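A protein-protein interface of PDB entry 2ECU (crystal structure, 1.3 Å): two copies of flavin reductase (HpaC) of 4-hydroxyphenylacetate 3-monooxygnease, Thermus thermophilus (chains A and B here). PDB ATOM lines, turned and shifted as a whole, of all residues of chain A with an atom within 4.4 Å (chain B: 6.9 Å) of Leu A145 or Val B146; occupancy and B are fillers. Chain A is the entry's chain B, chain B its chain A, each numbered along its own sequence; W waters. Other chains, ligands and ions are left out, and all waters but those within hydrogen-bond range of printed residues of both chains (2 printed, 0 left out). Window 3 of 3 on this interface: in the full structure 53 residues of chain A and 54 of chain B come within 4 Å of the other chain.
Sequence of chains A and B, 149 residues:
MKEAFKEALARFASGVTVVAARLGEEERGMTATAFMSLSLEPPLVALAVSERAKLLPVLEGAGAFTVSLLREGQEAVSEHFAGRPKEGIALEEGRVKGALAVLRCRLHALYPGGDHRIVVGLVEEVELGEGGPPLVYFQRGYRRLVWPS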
ATOM      1  N   PRO A 134      25.590  -1.944  -6.597  1.00  0.00           N
ATOM      2  CA  PRO A 134      24.423  -2.761  -6.256  1.00  0.00           C
ATOM      3  C   PRO A 134      24.644  -4.255  -6.090  1.00  0.00           C
ATOM      4  O   PRO A 134      25.684  -4.794  -6.458  1.00  0.00           O
ATOM      5  CB  PRO A 134      23.504  -2.492  -7.430  1.00  0.00           C
ATOM      6  CG  PRO A 134      24.496  -2.582  -8.582  1.00  0.00           C
ATOM      7  CD  PRO A 134      25.736  -1.840  -8.063  1.00  0.00           C
ATOM      8  N   VAL A 136      23.668  -7.718  -7.429  1.00  0.00           N
ATOM      9  CA  VAL A 136      23.184  -8.156  -8.729  1.00  0.00           C
ATOM     10  C   VAL A 136      22.955  -9.661  -8.733  1.00  0.00           C
ATOM     11  O   VAL A 136      23.635 -10.393  -8.014  1.00  0.00           O
ATOM     12  CB  VAL A 136      24.217  -7.806  -9.836  1.00  0.00           C
ATOM     13  CG1 VAL A 136      23.722  -8.261 -11.196  1.00  0.00           C
ATOM     14  CG2 VAL A 136      24.476  -6.312  -9.843  1.00  0.00           C
ATOM     15  N   ARG A 144      28.689  -9.014  -8.779  1.00  0.00           N
ATOM     16  CA  ARG A 144      29.109  -7.654  -8.502  1.00  0.00           C
ATOM     17  C   ARG A 144      29.431  -6.957  -9.814  1.00  0.00           C
ATOM     18  O   ARG A 144      29.796  -7.596 -10.805  1.00  0.00           O
ATOM     19  CB  ARG A 144      30.356  -7.652  -7.616  1.00  0.00           C
ATOM     20  CG  ARG A 144      30.115  -8.108  -6.187  1.00  0.00           C
ATOM     21  CD  ARG A 144      31.427  -8.187  -5.417  1.00  0.00           C
ATOM     22  NE  ARG A 144      32.243  -6.999  -5.642  1.00  0.00           N
ATOM     23  CZ  ARG A 144      33.434  -7.011  -6.234  1.00  0.00           C
ATOM     24  NH1 ARG A 144      33.959  -8.153  -6.656  1.00  0.00           N
ATOM     25  NH2 ARG A 144      34.089  -5.875  -6.425  1.00  0.00           N
ATOM     26  N   LEU A 145      29.290  -5.637  -9.819  1.00  0.00           N
ATOM     27  CA  LEU A 145      29.614  -4.847 -10.996  1.00  0.00           C
ATOM     28  C   LEU A 145      31.068  -4.411 -10.911  1.00  0.00           C
ATOM     29  O   LEU A 145      31.618  -4.255  -9.816  1.00  0.00           O
ATOM     30  CB  LEU A 145      28.771  -3.575 -11.050  1.00  0.00           C
ATOM     31  CG  LEU A 145      27.258  -3.618 -11.213  1.00  0.00           C
ATOM     32  CD1 LEU A 145      26.739  -2.187 -11.313  1.00  0.00           C
ATOM     33  CD2 LEU A 145      26.895  -4.400 -12.464  1.00  0.00           C
ATOM     34  N   VAL A 146      31.699  -4.241 -12.067  1.00  0.00           N
ATOM     35  CA  VAL A 146      33.058  -3.722 -12.096  1.00  0.00           C
ATOM     36  C   VAL A 146      32.725  -2.249 -11.868  1.00  0.00           C
ATOM     37  O   VAL A 146      32.047  -1.623 -12.685  1.00  0.00           O
ATOM     38  CB  VAL A 146      33.711  -3.938 -13.470  1.00  0.00           C
ATOM     39  CG1 VAL A 146      35.016  -3.175 -13.548  1.00  0.00           C
ATOM     40  CG2 VAL A 146      33.961  -5.428 -13.694  1.00  0.00           C
ATOM     41  N   TRP A 147      33.175  -1.707 -10.742  1.00  0.00           N
ATOM     42  CA  TRP A 147      32.836  -0.339 -10.374  1.00  0.00           C
ATOM     43  C   TRP A 147      33.969   0.332  -9.609  1.00  0.00           C
ATOM     44  O   TRP A 147      34.575  -0.278  -8.729  1.00  0.00           O
ATOM     45  CB  TRP A 147      31.566  -0.400  -9.517  1.00  0.00           C
ATOM     46  CG  TRP A 147      31.031   0.897  -9.037  1.00  0.00           C
ATOM     47  CD1 TRP A 147      31.304   1.512  -7.852  1.00  0.00           C
ATOM     48  CD2 TRP A 147      30.093   1.730  -9.719  1.00  0.00           C
ATOM     49  NE1 TRP A 147      30.587   2.679  -7.750  1.00  0.00           N
ATOM     50  CE2 TRP A 147      29.836   2.837  -8.885  1.00  0.00           C
ATOM     51  CE3 TRP A 147      29.444   1.647 -10.957  1.00  0.00           C
ATOM     52  CZ2 TRP A 147      28.953   3.860  -9.249  1.00  0.00           C
ATOM     53  CZ3 TRP A 147      28.569   2.662 -11.321  1.00  0.00           C
ATOM     54  CH2 TRP A 147      28.331   3.754 -10.468  1.00  0.00           C
ATOM     55  N   ALA B  13      20.077  -1.942 -11.178  1.00  0.00           N
ATOM     56  CA  ALA B  13      20.850  -2.475 -12.285  1.00  0.00           C
ATOM     57  C   ALA B  13      19.994  -3.444 -13.078  1.00  0.00           C
ATOM     58  O   ALA B  13      19.109  -4.097 -12.535  1.00  0.00           O
ATOM     59  CB  ALA B  13      22.077  -3.194 -11.755  1.00  0.00           C
ATOM     60  N   PRO B 133      29.393 -12.989 -20.125  1.00  0.00           N
ATOM     61  CA  PRO B 133      28.821 -11.868 -19.378  1.00  0.00           C
ATOM     62  C   PRO B 133      27.820 -11.049 -20.185  1.00  0.00           C
ATOM     63  O   PRO B 133      27.873 -11.014 -21.414  1.00  0.00           O
ATOM     64  CB  PRO B 133      30.053 -11.071 -18.960  1.00  0.00           C
ATOM     65  CG  PRO B 133      30.986 -11.293 -20.095  1.00  0.00           C
ATOM     66  CD  PRO B 133      30.831 -12.772 -20.366  1.00  0.00           C
ATOM     67  N   VAL B 136      25.062  -4.564 -19.113  1.00  0.00           N
ATOM     68  CA  VAL B 136      24.326  -4.082 -17.954  1.00  0.00           C
ATOM     69  C   VAL B 136      24.202  -2.571 -17.982  1.00  0.00           C
ATOM     70  O   VAL B 136      25.093  -1.878 -18.471  1.00  0.00           O
ATOM     71  CB  VAL B 136      25.041  -4.490 -16.635  1.00  0.00           C
ATOM     72  CG1 VAL B 136      24.231  -4.035 -15.431  1.00  0.00           C
ATOM     73  CG2 VAL B 136      25.245  -5.995 -16.600  1.00  0.00           C
ATOM     74  N   TYR B 137      23.085  -2.064 -17.467  1.00  0.00           N
ATOM     75  CA  TYR B 137      22.876  -0.623 -17.394  1.00  0.00           C
ATOM     76  C   TYR B 137      22.659  -0.291 -15.924  1.00  0.00           C
ATOM     77  O   TYR B 137      21.853  -0.928 -15.244  1.00  0.00           O
ATOM     78  CB  TYR B 137      21.659  -0.189 -18.213  1.00  0.00           C
ATOM     79  CG  TYR B 137      21.735   1.263 -18.626  1.00  0.00           C
ATOM     80  CD1 TYR B 137      22.678   1.688 -19.562  1.00  0.00           C
ATOM     81  CD2 TYR B 137      20.897   2.220 -18.054  1.00  0.00           C
ATOM     82  CE1 TYR B 137      22.790   3.028 -19.919  1.00  0.00           C
ATOM     83  CE2 TYR B 137      21.001   3.569 -18.406  1.00  0.00           C
ATOM     84  CZ  TYR B 137      21.951   3.962 -19.338  1.00  0.00           C
ATOM     85  OH  TYR B 137      22.072   5.292 -19.679  1.00  0.00           O
ATOM     86  N   PHE B 138      23.396   0.697 -15.435  1.00  0.00           N
ATOM     87  CA  PHE B 138      23.312   1.104 -14.038  1.00  0.00           C
ATOM     88  C   PHE B 138      23.917   2.494 -13.922  1.00  0.00           C
ATOM     89  O   PHE B 138      24.960   2.771 -14.511  1.00  0.00           O
ATOM     90  CB  PHE B 138      24.098   0.116 -13.168  1.00  0.00           C
ATOM     91  CG  PHE B 138      24.200   0.516 -11.716  1.00  0.00           C
ATOM     92  CD1 PHE B 138      23.120   0.368 -10.849  1.00  0.00           C
ATOM     93  CD2 PHE B 138      25.393   1.028 -11.211  1.00  0.00           C
ATOM     94  CE1 PHE B 138      23.229   0.722  -9.500  1.00  0.00           C
ATOM     95  CE2 PHE B 138      25.509   1.384  -9.868  1.00  0.00           C
ATOM     96  CZ  PHE B 138      24.427   1.230  -9.011  1.00  0.00           C
ATOM     97  N   GLN B 139      23.265   3.361 -13.157  1.00  0.00           N
ATOM     98  CA  GLN B 139      23.743   4.725 -12.977  1.00  0.00           C
ATOM     99  C   GLN B 139      24.076   5.428 -14.290  1.00  0.00           C
ATOM    100  O   GLN B 139      25.180   5.939 -14.483  1.00  0.00           O
ATOM    101  CB  GLN B 139      24.950   4.752 -12.033  1.00  0.00           C
ATOM    102  CG  GLN B 139      24.564   4.683 -10.564  1.00  0.00           C
ATOM    103  CD  GLN B 139      23.771   5.897 -10.106  1.00  0.00           C
ATOM    104  OE1 GLN B 139      23.405   6.756 -10.910  1.00  0.00           O
ATOM    105  NE2 GLN B 139      23.503   5.975  -8.808  1.00  0.00           N
ATOM    106  N   ARG B 143      27.599  -0.931 -17.909  1.00  0.00           N
ATOM    107  CA  ARG B 143      28.542  -1.493 -16.958  1.00  0.00           C
ATOM    108  C   ARG B 143      28.844  -2.944 -17.269  1.00  0.00           C
ATOM    109  O   ARG B 143      28.124  -3.595 -18.027  1.00  0.00           O
ATOM    110  CB  ARG B 143      27.967  -1.408 -15.542  1.00  0.00           C
ATOM    111  CG  ARG B 143      27.384  -0.059 -15.171  1.00  0.00           C
ATOM    112  CD  ARG B 143      28.425   1.042 -15.192  1.00  0.00           C
ATOM    113  NE  ARG B 143      27.821   2.340 -14.917  1.00  0.00           N
ATOM    114  CZ  ARG B 143      28.506   3.462 -14.729  1.00  0.00           C
ATOM    115  NH1 ARG B 143      29.833   3.451 -14.786  1.00  0.00           N
ATOM    116  NH2 ARG B 143      27.865   4.596 -14.484  1.00  0.00           N
ATOM    117  N   ARG B 144      29.915  -3.447 -16.669  1.00  0.00           N
ATOM    118  CA  ARG B 144      30.327  -4.827 -16.857  1.00  0.00           C
ATOM    119  C   ARG B 144      30.300  -5.535 -15.509  1.00  0.00           C
ATOM    120  O   ARG B 144      30.503  -4.911 -14.465  1.00  0.00           O
ATOM    121  CB  ARG B 144      31.741  -4.874 -17.442  1.00  0.00           C
ATOM    122  CG  ARG B 144      31.871  -4.098 -18.745  1.00  0.00           C
ATOM    123  CD  ARG B 144      33.288  -4.115 -19.295  1.00  0.00           C
ATOM    124  NE  ARG B 144      33.406  -3.293 -20.497  1.00  0.00           N
ATOM    125  CZ  ARG B 144      33.428  -1.963 -20.507  1.00  0.00           C
ATOM    126  NH1 ARG B 144      33.345  -1.279 -19.372  1.00  0.00           N
ATOM    127  NH2 ARG B 144      33.524  -1.313 -21.657  1.00  0.00           N
ATOM    128  N   LEU B 145      30.020  -6.830 -15.527  1.00  0.00           N
ATOM    129  CA  LEU B 145      30.006  -7.612 -14.298  1.00  0.00           C
ATOM    130  C   LEU B 145      31.402  -8.138 -14.023  1.00  0.00           C
ATOM    131  O   LEU B 145      32.200  -8.326 -14.947  1.00  0.00           O
ATOM    132  CB  LEU B 145      29.090  -8.829 -14.423  1.00  0.00           C
ATOM    133  CG  LEU B 145      27.579  -8.679 -14.529  1.00  0.00           C
ATOM    134  CD1 LEU B 145      26.960 -10.072 -14.520  1.00  0.00           C
ATOM    135  CD2 LEU B 145      27.053  -7.860 -13.364  1.00  0.00           C
ATOM    136  N   VAL B 146      31.700  -8.363 -12.749  1.00  0.00           N
ATOM    137  CA  VAL B 146      32.972  -8.960 -12.381  1.00  0.00           C
ATOM    138  C   VAL B 146      32.731 -10.388 -12.867  1.00  0.00           C
ATOM    139  O   VAL B 146      31.833 -11.079 -12.378  1.00  0.00           O
ATOM    140  CB  VAL B 146      33.189  -8.934 -10.856  1.00  0.00           C
ATOM    141  CG1 VAL B 146      34.354  -9.834 -10.479  1.00  0.00           C
ATOM    142  CG2 VAL B 146      33.468  -7.509 -10.399  1.00  0.00           C
ATOM    143  N   TRP B 147      33.519 -10.814 -13.847  1.00  0.00           N
ATOM    144  CA  TRP B 147      33.357 -12.130 -14.459  1.00  0.00           C
ATOM    145  C   TRP B 147      34.734 -12.542 -14.976  1.00  0.00           C
ATOM    146  O   TRP B 147      34.958 -12.630 -16.181  1.00  0.00           O
ATOM    147  CB  TRP B 147      32.356 -11.982 -15.610  1.00  0.00           C
ATOM    148  CG  TRP B 147      31.750 -13.237 -16.138  1.00  0.00           C
ATOM    149  CD1 TRP B 147      32.141 -13.934 -17.240  1.00  0.00           C
ATOM    150  CD2 TRP B 147      30.584 -13.901 -15.634  1.00  0.00           C
ATOM    151  NE1 TRP B 147      31.285 -14.991 -17.463  1.00  0.00           N
ATOM    152  CE2 TRP B 147      30.321 -14.991 -16.491  1.00  0.00           C
ATOM    153  CE3 TRP B 147      29.737 -13.678 -14.543  1.00  0.00           C
ATOM    154  CZ2 TRP B 147      29.242 -15.859 -16.292  1.00  0.00           C
ATOM    155  CZ3 TRP B 147      28.663 -14.541 -14.345  1.00  0.00           C
ATOM    156  CH2 TRP B 147      28.427 -15.618 -15.216  1.00  0.00           C
ATOM    157  N   PRO B 148      35.674 -12.805 -14.060  1.00  0.00           N
ATOM    158  CA  PRO B 148      37.035 -13.195 -14.428  1.00  0.00           C
ATOM    159  C   PRO B 148      37.240 -14.634 -14.870  1.00  0.00           C
ATOM    160  O   PRO B 148      36.422 -15.515 -14.603  1.00  0.00           O
ATOM    161  CB  PRO B 148      37.826 -12.875 -13.169  1.00  0.00           C
ATOM    162  CG  PRO B 148      36.866 -13.255 -12.095  1.00  0.00           C
ATOM    163  CD  PRO B 148      35.546 -12.683 -12.594  1.00  0.00           C
HETATM  164  O   HOH W   1      30.408 -11.080 -10.005  1.00  0.00           O
HETATM  165  O   HOH W   2      31.675  -1.447 -15.381  1.00  0.00           O
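The backbone carbonyl oxygen of Arg A144 sits at hydrogen-bond distance from the backbone NH of Val B146 (2.8 Å). The backbone carbonyl oxygen (O) of Arg B144 lies within hydrogen-bond range of the backbone NH (N) of Val A146 (2.8 Å).
The backbone carbonyl oxygen of Phe B138 lies within hydrogen-bond range of the guanidinium group of Arg B143 (2.9 Å). The backbone carbonyl oxygen (O) of Val B136 is in hydrogen-bond range of the backbone NH (N) of Arg B143, at 2.7 Å. The guanidinium group of Arg B143 is in hydrogen-bond range of the backbone carbonyl oxygen of Gln B139, 3.0 Å away.
Among the printed residues, merely in contact across the chains: Pro A134 with Phe B138 (3.5 Å), Leu A145 with Phe B138 (3.5 Å), Arg A144 with Leu B145 (3.5 Å), Trp A147 with Arg B143 (3.5 Å), Trp A147 with Phe B138 (3.6 Å), Leu A145 with Leu B145 (3.6 Å), Leu A145 with Arg B144 (3.6 Å), Val A146 with Leu B145 (3.6 Å), Leu A145 with Val B146 (3.8 Å), Val A146 with Val B146 (3.8 Å), Trp A147 with Gln B139 (3.9 Å) and Val A136 with Leu B145 (3.99 Å).
Printed residues of chain B within 4 Å of Leu A145: Phe B138 (3.5 Å), Arg B144 (3.6 Å), Leu B145 (3.6 Å) and Val B146 (3.8 Å). Val B146 touches just these residues of chain A: Arg A144, Leu A145 and Val A146. Printed residues of chain A within 4 Å of Gln B139: Trp A147. Of the printed residues of chain B, Arg A144 touches Leu B145 (3.5 Å) and Val B146 (2.8 Å). Printed residues of chain A within 4 Å of Phe B138: Pro A134, Leu A145 and Trp A147. Pro B148 touches none of the printed residues of chain A. The nearest printed residue of chain B that does not touch Leu A145 is Val B136 (4.004 Å). The nearest printed residue of chain A that does not touch Val B146 is Trp A147 (5.8 Å). The nearest printed residue of chain A that does not touch Gln B139 is Leu A145 (6.8 Å).
Of the 12 printed residues of chain B, 6 touch a printed residue of chain A. Printed residues of chain B that touch a printed residue of chain A: Phe B138, Gln B139, Arg B143, Arg B144, Leu B145 and Val B146. Among the printed residues, no Asp or Glu carboxylate lies within 4 Å of a Lys or Arg side-chain nitrogen of the other chain.
Val A136 touches Leu B145, but with the chains exchanged Leu A145 does not touch Val B136 (4.004 Å). Leu A145 touches its own counterpart, Leu B145. Leu A145 touches Val B146, and with the chains exchanged Val A146 touches Leu B145. Val B146 touches its own counterpart, Val A146.
Water W2 bridges O of Val A146 (2.7 Å) and N of Arg B144 (3.0 Å). Water W1 bridges O of Val B146 (2.8 Å) and N of Arg A144 (3.0 Å).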
